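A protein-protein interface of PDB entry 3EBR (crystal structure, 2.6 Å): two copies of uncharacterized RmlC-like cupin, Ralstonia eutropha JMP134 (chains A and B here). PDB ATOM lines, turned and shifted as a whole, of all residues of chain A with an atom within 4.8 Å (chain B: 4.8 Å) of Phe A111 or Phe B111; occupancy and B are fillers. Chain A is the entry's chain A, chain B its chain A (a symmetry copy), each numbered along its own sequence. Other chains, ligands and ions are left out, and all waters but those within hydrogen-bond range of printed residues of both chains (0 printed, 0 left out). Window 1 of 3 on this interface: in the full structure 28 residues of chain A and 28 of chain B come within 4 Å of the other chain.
Printed residues of chain A that touch a printed residue of chain B: Ile A44, Leu A46, Ile A65, Tyr A67, Val A69, Val A87, Phe A111 and Ile A113. Hydrophobic or aromatic side chains of chain A that line the printed part of chain B: Ile A44, Leu A46, Ile A65, Tyr A67, Val A69, Val A87, Phe A111 and Ile A113. Of the 13 printed residues of chain B, 8 touch a printed residue of chain A. Printed residues of chain B that touch a printed residue of chain A: Ile B44, Leu B46, Ile B65, Tyr B67, Val B69, Val B87, Phe B111 and Ile B113. Hydrophobic or aromatic side chains of chain B that line the printed part of chain A: Ile B44, Leu B46, Ile B65, Tyr B67, Val B69, Val B87, Phe B111 and Ile B113.
Of the printed residues of chain B, Ile A65 touches Ile B44 and Ile B113. Of the printed residues of chain B, Val A87 touches Phe B111 (3.6 Å). Phe A111 touches three residues of chain B. Of the printed residues of chain A, Leu B46 touches Tyr A67. Of chain A, only Tyr A67, Val A87 and Phe A111 come within 4 Å of Phe B111. The nearest residue of chain B that does not touch Phe A111 is Ile B65 (4.1 Å). The nearest printed residue of chain A that does not touch Val B69 is Val A69 (5.6 Å).
Ile A65 touches Ile B113, and with the chains exchanged Ile A113 touches Ile B65. Tyr A67 touches Phe B111, and with the chains exchanged Phe A111 touches Tyr B67. Val A87 touches Phe B111, and with the chains exchanged Phe A111 touches Val B87. Ile B113 touches its own counterpart, Ile A113.
N of Ile A65 lies within hydrogen-bond range of O of Ile A113, at 2.9 Å. N of Phe A111 sits at hydrogen-bond distance from O of Tyr A67. The backbone NH of Val A69 lies within hydrogen-bond range of the backbone carbonyl oxygen of Ile A109, at 3.0 Å. The backbone NH (N) of Ile B65 is in hydrogen-bond range of the backbone carbonyl oxygen (O) of Ile B113 (2.9 Å). N of Phe B111 is in hydrogen-bond range of O of Tyr B67 (2.7 Å). The backbone NH (N) of Val B69 is in hydrogen-bond range of the backbone carbonyl oxygen (O) of Ile B109 (3.0 Å).
Among the printed residues, pairs that only touch across the chains: Ile A113 with Ile B113, Ile A113 with Ile B65, Ile A65 with Ile B113, Val A87 with Phe B111, Phe A111 with Val B87, Ile A44 with Ile B65, Ile A65 with Ile B44, Phe A111 with Tyr B67, Tyr A67 with Phe B111, Phe A111 with Phe B111, Tyr A67 with Leu B46, Leu A46 with Tyr B67, Val A69 with Tyr B67 and Tyr A67 with Val B69.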
ATOM      1  N   ILE A  44       4.636  14.027 -18.817  1.00  0.00           N
ATOM      2  CA  ILE A  44       5.487  14.997 -19.506  1.00  0.00           C
ATOM      3  C   ILE A  44       4.929  15.024 -20.925  1.00  0.00           C
ATOM      4  O   ILE A  44       4.858  13.980 -21.568  1.00  0.00           O
ATOM      5  CB  ILE A  44       6.975  14.638 -19.501  1.00  0.00           C
ATOM      6  CG1 ILE A  44       7.525  14.579 -18.068  1.00  0.00           C
ATOM      7  CG2 ILE A  44       7.764  15.671 -20.299  1.00  0.00           C
ATOM      8  CD1 ILE A  44       9.016  14.210 -17.977  1.00  0.00           C
ATOM      9  N   THR A  45       4.482  16.186 -21.389  1.00  0.00           N
ATOM     10  CA  THR A  45       3.904  16.321 -22.729  1.00  0.00           C
ATOM     11  C   THR A  45       4.147  17.648 -23.420  1.00  0.00           C
ATOM     12  O   THR A  45       4.553  18.607 -22.782  1.00  0.00           O
ATOM     13  CB  THR A  45       2.341  16.212 -22.668  1.00  0.00           C
ATOM     14  OG1 THR A  45       1.831  17.246 -21.817  1.00  0.00           O
ATOM     15  CG2 THR A  45       1.863  14.877 -22.143  1.00  0.00           C
ATOM     16  N   LEU A  46       3.946  17.649 -24.738  1.00  0.00           N
ATOM     17  CA  LEU A  46       3.945  18.849 -25.577  1.00  0.00           C
ATOM     18  C   LEU A  46       2.462  18.950 -25.833  1.00  0.00           C
ATOM     19  O   LEU A  46       1.803  17.914 -25.992  1.00  0.00           O
ATOM     20  CB  LEU A  46       4.732  18.747 -26.875  1.00  0.00           C
ATOM     21  CG  LEU A  46       6.250  18.925 -26.812  1.00  0.00           C
ATOM     22  CD1 LEU A  46       6.876  18.477 -28.108  1.00  0.00           C
ATOM     23  CD2 LEU A  46       6.619  20.375 -26.493  1.00  0.00           C
ATOM     24  N   ILE A  65       4.443  22.509 -14.309  1.00  0.00           N
ATOM     25  CA  ILE A  65       5.530  23.351 -14.780  1.00  0.00           C
ATOM     26  C   ILE A  65       5.236  23.501 -16.273  1.00  0.00           C
ATOM     27  O   ILE A  65       5.120  22.485 -16.958  1.00  0.00           O
ATOM     28  CB  ILE A  65       6.895  22.715 -14.597  1.00  0.00           C
ATOM     29  CG1 ILE A  65       7.209  22.524 -13.104  1.00  0.00           C
ATOM     30  CG2 ILE A  65       7.980  23.579 -15.269  1.00  0.00           C
ATOM     31  CD1 ILE A  65       8.491  21.774 -12.838  1.00  0.00           C
ATOM     32  N   VAL A  66       5.078  24.730 -16.766  1.00  0.00           N
ATOM     33  CA  VAL A  66       4.800  24.974 -18.174  1.00  0.00           C
ATOM     34  C   VAL A  66       5.869  25.865 -18.804  1.00  0.00           C
ATOM     35  O   VAL A  66       6.070  26.980 -18.335  1.00  0.00           O
ATOM     36  CB  VAL A  66       3.435  25.672 -18.407  1.00  0.00           C
ATOM     37  CG1 VAL A  66       3.198  25.827 -19.894  1.00  0.00           C
ATOM     38  CG2 VAL A  66       2.287  24.902 -17.783  1.00  0.00           C
ATOM     39  N   TYR A  67       6.566  25.343 -19.823  1.00  0.00           N
ATOM     40  CA  TYR A  67       7.543  26.078 -20.611  1.00  0.00           C
ATOM     41  C   TYR A  67       6.869  26.313 -21.975  1.00  0.00           C
ATOM     42  O   TYR A  67       6.531  25.354 -22.673  1.00  0.00           O
ATOM     43  CB  TYR A  67       8.859  25.337 -20.785  1.00  0.00           C
ATOM     44  CG  TYR A  67       9.772  26.047 -21.759  1.00  0.00           C
ATOM     45  CD1 TYR A  67      10.422  27.219 -21.396  1.00  0.00           C
ATOM     46  CD2 TYR A  67       9.960  25.565 -23.054  1.00  0.00           C
ATOM     47  CE1 TYR A  67      11.253  27.899 -22.299  1.00  0.00           C
ATOM     48  CE2 TYR A  67      10.783  26.240 -23.967  1.00  0.00           C
ATOM     49  CZ  TYR A  67      11.431  27.397 -23.575  1.00  0.00           C
ATOM     50  OH  TYR A  67      12.244  28.048 -24.460  1.00  0.00           O
ATOM     51  N   VAL A  69       6.886  26.941 -25.664  1.00  0.00           N
ATOM     52  CA  VAL A  69       7.789  26.749 -26.807  1.00  0.00           C
ATOM     53  C   VAL A  69       7.491  27.857 -27.818  1.00  0.00           C
ATOM     54  O   VAL A  69       8.422  28.482 -28.330  1.00  0.00           O
ATOM     55  CB  VAL A  69       7.681  25.331 -27.384  1.00  0.00           C
ATOM     56  CG1 VAL A  69       8.635  25.153 -28.537  1.00  0.00           C
ATOM     57  CG2 VAL A  69       8.005  24.313 -26.299  1.00  0.00           C
ATOM     58  N   VAL A  87       8.335  30.610 -18.289  1.00  0.00           N
ATOM     59  CA  VAL A  87       8.085  29.461 -17.430  1.00  0.00           C
ATOM     60  C   VAL A  87       6.967  29.827 -16.460  1.00  0.00           C
ATOM     61  O   VAL A  87       7.069  30.851 -15.785  1.00  0.00           O
ATOM     62  CB  VAL A  87       9.322  29.010 -16.617  1.00  0.00           C
ATOM     63  CG1 VAL A  87       8.945  27.899 -15.616  1.00  0.00           C
ATOM     64  CG2 VAL A  87      10.402  28.532 -17.529  1.00  0.00           C
ATOM     65  N   ILE A 109       2.241  26.226 -28.488  1.00  0.00           N
ATOM     66  CA  ILE A 109       2.909  24.951 -28.218  1.00  0.00           C
ATOM     67  C   ILE A 109       3.484  25.126 -26.820  1.00  0.00           C
ATOM     68  O   ILE A 109       4.151  26.135 -26.567  1.00  0.00           O
ATOM     69  CB  ILE A 109       4.058  24.613 -29.184  1.00  0.00           C
ATOM     70  CG1 ILE A 109       3.645  24.722 -30.666  1.00  0.00           C
ATOM     71  CG2 ILE A 109       4.595  23.199 -28.877  1.00  0.00           C
ATOM     72  CD1 ILE A 109       2.622  23.738 -31.097  1.00  0.00           C
ATOM     73  N   THR A 110       3.235  24.178 -25.915  1.00  0.00           N
ATOM     74  CA  THR A 110       3.753  24.243 -24.538  1.00  0.00           C
ATOM     75  C   THR A 110       4.297  22.907 -24.068  1.00  0.00           C
ATOM     76  O   THR A 110       3.699  21.880 -24.360  1.00  0.00           O
ATOM     77  CB  THR A 110       2.660  24.673 -23.524  1.00  0.00           C
ATOM     78  OG1 THR A 110       1.601  23.704 -23.501  1.00  0.00           O
ATOM     79  CG2 THR A 110       2.098  26.049 -23.875  1.00  0.00           C
ATOM     80  N   PHE A 111       5.420  22.939 -23.344  1.00  0.00           N
ATOM     81  CA  PHE A 111       6.063  21.762 -22.763  1.00  0.00           C
ATOM     82  C   PHE A 111       5.577  21.774 -21.329  1.00  0.00           C
ATOM     83  O   PHE A 111       5.897  22.695 -20.595  1.00  0.00           O
ATOM     84  CB  PHE A 111       7.578  21.821 -22.848  1.00  0.00           C
ATOM     85  CG  PHE A 111       8.255  20.677 -22.160  1.00  0.00           C
ATOM     86  CD1 PHE A 111       8.206  19.405 -22.712  1.00  0.00           C
ATOM     87  CD2 PHE A 111       8.965  20.866 -20.975  1.00  0.00           C
ATOM     88  CE1 PHE A 111       8.826  18.335 -22.091  1.00  0.00           C
ATOM     89  CE2 PHE A 111       9.605  19.790 -20.350  1.00  0.00           C
ATOM     90  CZ  PHE A 111       9.522  18.523 -20.905  1.00  0.00           C
ATOM     91  N   ASN A 112       4.837  20.736 -20.946  1.00  0.00           N
ATOM     92  CA  ASN A 112       4.204  20.619 -19.646  1.00  0.00           C
ATOM     93  C   ASN A 112       4.665  19.424 -18.841  1.00  0.00           C
ATOM     94  O   ASN A 112       4.871  18.365 -19.418  1.00  0.00           O
ATOM     95  CB  ASN A 112       2.712  20.435 -19.879  1.00  0.00           C
ATOM     96  CG  ASN A 112       2.175  21.377 -20.917  1.00  0.00           C
ATOM     97  OD1 ASN A 112       2.244  22.595 -20.773  1.00  0.00           O
ATOM     98  ND2 ASN A 112       1.644  20.812 -21.988  1.00  0.00           N
ATOM     99  N   ILE A 113       4.826  19.608 -17.527  1.00  0.00           N
ATOM    100  CA  ILE A 113       5.188  18.556 -16.584  1.00  0.00           C
ATOM    101  C   ILE A 113       4.086  18.694 -15.551  1.00  0.00           C
ATOM    102  O   ILE A 113       4.129  19.611 -14.741  1.00  0.00           O
ATOM    103  CB  ILE A 113       6.571  18.711 -15.978  1.00  0.00           C
ATOM    104  CG1 ILE A 113       7.609  18.719 -17.097  1.00  0.00           C
ATOM    105  CG2 ILE A 113       6.832  17.581 -14.975  1.00  0.00           C
ATOM    106  CD1 ILE A 113       8.989  18.624 -16.609  1.00  0.00           C
ATOM    107  N   ILE B  44      14.996  25.201 -12.183  1.00  0.00           N
ATOM    108  CA  ILE B  44      14.395  25.200 -13.517  1.00  0.00           C
ATOM    109  C   ILE B  44      15.222  26.224 -14.287  1.00  0.00           C
ATOM    110  O   ILE B  44      15.319  27.371 -13.859  1.00  0.00           O
ATOM    111  CB  ILE B  44      12.907  25.565 -13.531  1.00  0.00           C
ATOM    112  CG1 ILE B  44      12.082  24.549 -12.726  1.00  0.00           C
ATOM    113  CG2 ILE B  44      12.394  25.602 -14.967  1.00  0.00           C
ATOM    114  CD1 ILE B  44      10.575  24.853 -12.681  1.00  0.00           C
ATOM    115  N   THR B  45      15.860  25.806 -15.375  1.00  0.00           N
ATOM    116  CA  THR B  45      16.701  26.698 -16.177  1.00  0.00           C
ATOM    117  C   THR B  45      16.727  26.416 -17.667  1.00  0.00           C
ATOM    118  O   THR B  45      16.295  25.359 -18.099  1.00  0.00           O
ATOM    119  CB  THR B  45      18.204  26.572 -15.748  1.00  0.00           C
ATOM    120  OG1 THR B  45      18.631  25.216 -15.928  1.00  0.00           O
ATOM    121  CG2 THR B  45      18.440  26.964 -14.306  1.00  0.00           C
ATOM    122  N   LEU B  46      17.183  27.412 -18.427  1.00  0.00           N
ATOM    123  CA  LEU B  46      17.464  27.302 -19.860  1.00  0.00           C
ATOM    124  C   LEU B  46      18.971  27.294 -19.800  1.00  0.00           C
ATOM    125  O   LEU B  46      19.548  28.008 -18.967  1.00  0.00           O
ATOM    126  CB  LEU B  46      16.943  28.441 -20.724  1.00  0.00           C
ATOM    127  CG  LEU B  46      15.467  28.423 -21.123  1.00  0.00           C
ATOM    128  CD1 LEU B  46      15.069  29.764 -21.687  1.00  0.00           C
ATOM    129  CD2 LEU B  46      15.180  27.298 -22.119  1.00  0.00           C
ATOM    130  N   ILE B  65      15.098  16.361 -15.946  1.00  0.00           N
ATOM    131  CA  ILE B  65      14.209  16.296 -17.095  1.00  0.00           C
ATOM    132  C   ILE B  65      14.806  17.323 -18.057  1.00  0.00           C
ATOM    133  O   ILE B  65      14.959  18.481 -17.668  1.00  0.00           O
ATOM    134  CB  ILE B  65      12.781  16.686 -16.763  1.00  0.00           C
ATOM    135  CG1 ILE B  65      12.162  15.686 -15.774  1.00  0.00           C
ATOM    136  CG2 ILE B  65      11.938  16.761 -18.052  1.00  0.00           C
ATOM    137  CD1 ILE B  65      10.787  16.075 -15.289  1.00  0.00           C
ATOM    138  N   VAL B  66      15.174  16.914 -19.272  1.00  0.00           N
ATOM    139  CA  VAL B  66      15.747  17.818 -20.259  1.00  0.00           C
ATOM    140  C   VAL B  66      14.913  17.842 -21.538  1.00  0.00           C
ATOM    141  O   VAL B  66      14.730  16.797 -22.152  1.00  0.00           O
ATOM    142  CB  VAL B  66      17.191  17.428 -20.668  1.00  0.00           C
ATOM    143  CG1 VAL B  66      17.730  18.453 -21.642  1.00  0.00           C
ATOM    144  CG2 VAL B  66      18.115  17.324 -19.469  1.00  0.00           C
ATOM    145  N   TYR B  67      14.385  19.023 -21.892  1.00  0.00           N
ATOM    146  CA  TYR B  67      13.658  19.259 -23.129  1.00  0.00           C
ATOM    147  C   TYR B  67      14.607  20.097 -24.004  1.00  0.00           C
ATOM    148  O   TYR B  67      14.984  21.208 -23.621  1.00  0.00           O
ATOM    149  CB  TYR B  67      12.337  19.985 -22.923  1.00  0.00           C
ATOM    150  CG  TYR B  67      11.706  20.374 -24.241  1.00  0.00           C
ATOM    151  CD1 TYR B  67      11.111  19.417 -25.053  1.00  0.00           C
ATOM    152  CD2 TYR B  67      11.733  21.693 -24.692  1.00  0.00           C
ATOM    153  CE1 TYR B  67      10.543  19.762 -26.288  1.00  0.00           C
ATOM    154  CE2 TYR B  67      11.175  22.048 -25.929  1.00  0.00           C
ATOM    155  CZ  TYR B  67      10.574  21.079 -26.711  1.00  0.00           C
ATOM    156  OH  TYR B  67      10.018  21.427 -27.909  1.00  0.00           O
ATOM    157  N   VAL B  69      15.379  22.544 -26.728  1.00  0.00           N
ATOM    158  CA  VAL B  69      14.705  23.632 -27.451  1.00  0.00           C
ATOM    159  C   VAL B  69      15.301  23.684 -28.858  1.00  0.00           C
ATOM    160  O   VAL B  69      14.553  23.772 -29.835  1.00  0.00           O
ATOM    161  CB  VAL B  69      14.790  24.960 -26.687  1.00  0.00           C
ATOM    162  CG1 VAL B  69      14.071  26.051 -27.437  1.00  0.00           C
ATOM    163  CG2 VAL B  69      14.164  24.797 -25.309  1.00  0.00           C
ATOM    164  N   VAL B  87      12.855  14.688 -25.368  1.00  0.00           N
ATOM    165  CA  VAL B  87      12.821  14.727 -23.913  1.00  0.00           C
ATOM    166  C   VAL B  87      13.754  13.642 -23.386  1.00  0.00           C
ATOM    167  O   VAL B  87      13.618  12.487 -23.786  1.00  0.00           O
ATOM    168  CB  VAL B  87      11.409  14.502 -23.318  1.00  0.00           C
ATOM    169  CG1 VAL B  87      11.474  14.396 -21.781  1.00  0.00           C
ATOM    170  CG2 VAL B  87      10.491  15.608 -23.716  1.00  0.00           C
ATOM    171  N   ILE B 109      20.402  24.730 -26.970  1.00  0.00           N
ATOM    172  CA  ILE B 109      19.576  25.390 -25.957  1.00  0.00           C
ATOM    173  C   ILE B 109      18.754  24.257 -25.357  1.00  0.00           C
ATOM    174  O   ILE B 109      18.149  23.490 -26.113  1.00  0.00           O
ATOM    175  CB  ILE B 109      18.613  26.456 -26.509  1.00  0.00           C
ATOM    176  CG1 ILE B 109      19.320  27.490 -27.410  1.00  0.00           C
ATOM    177  CG2 ILE B 109      17.895  27.162 -25.339  1.00  0.00           C
ATOM    178  CD1 ILE B 109      20.309  28.346 -26.711  1.00  0.00           C
ATOM    179  N   THR B 110      18.729  24.134 -24.029  1.00  0.00           N
ATOM    180  CA  THR B 110      17.958  23.081 -23.346  1.00  0.00           C
ATOM    181  C   THR B 110      17.207  23.614 -22.140  1.00  0.00           C
ATOM    182  O   THR B 110      17.750  24.429 -21.409  1.00  0.00           O
ATOM    183  CB  THR B 110      18.864  21.926 -22.847  1.00  0.00           C
ATOM    184  OG1 THR B 110      19.801  22.419 -21.877  1.00  0.00           O
ATOM    185  CG2 THR B 110      19.612  21.275 -24.009  1.00  0.00           C
ATOM    186  N   PHE B 111      15.971  23.142 -21.948  1.00  0.00           N
ATOM    187  CA  PHE B 111      15.118  23.498 -20.816  1.00  0.00           C
ATOM    188  C   PHE B 111      15.309  22.340 -19.860  1.00  0.00           C
ATOM    189  O   PHE B 111      14.940  21.223 -20.188  1.00  0.00           O
ATOM    190  CB  PHE B 111      13.661  23.669 -21.213  1.00  0.00           C
ATOM    191  CG  PHE B 111      12.757  23.925 -20.048  1.00  0.00           C
ATOM    192  CD1 PHE B 111      12.793  25.148 -19.393  1.00  0.00           C
ATOM    193  CD2 PHE B 111      11.848  22.961 -19.616  1.00  0.00           C
ATOM    194  CE1 PHE B 111      11.964  25.403 -18.315  1.00  0.00           C
ATOM    195  CE2 PHE B 111      10.998  23.218 -18.535  1.00  0.00           C
ATOM    196  CZ  PHE B 111      11.068  24.437 -17.879  1.00  0.00           C
ATOM    197  N   ASN B 112      15.857  22.629 -18.682  1.00  0.00           N
ATOM    198  CA  ASN B 112      16.207  21.641 -17.679  1.00  0.00           C
ATOM    199  C   ASN B 112      15.484  21.819 -16.362  1.00  0.00           C
ATOM    200  O   ASN B 112      15.297  22.950 -15.936  1.00  0.00           O
ATOM    201  CB  ASN B 112      17.691  21.796 -17.383  1.00  0.00           C
ATOM    202  CG  ASN B 112      18.509  21.950 -18.632  1.00  0.00           C
ATOM    203  OD1 ASN B 112      18.529  21.077 -19.496  1.00  0.00           O
ATOM    204  ND2 ASN B 112      19.186  23.081 -18.741  1.00  0.00           N
ATOM    205  N   ILE B 113      15.085  20.706 -15.738  1.00  0.00           N
ATOM    206  CA  ILE B 113      14.445  20.677 -14.428  1.00  0.00           C
ATOM    207  C   ILE B 113      15.330  19.690 -13.689  1.00  0.00           C
ATOM    208  O   ILE B 113      15.215  18.491 -13.913  1.00  0.00           O
ATOM    209  CB  ILE B 113      12.991  20.244 -14.453  1.00  0.00           C
ATOM    210  CG1 ILE B 113      12.200  21.198 -15.343  1.00  0.00           C
ATOM    211  CG2 ILE B 113      12.431  20.209 -13.026  1.00  0.00           C
ATOM    212  CD1 ILE B 113      10.749  21.014 -15.246  1.00  0.00           C
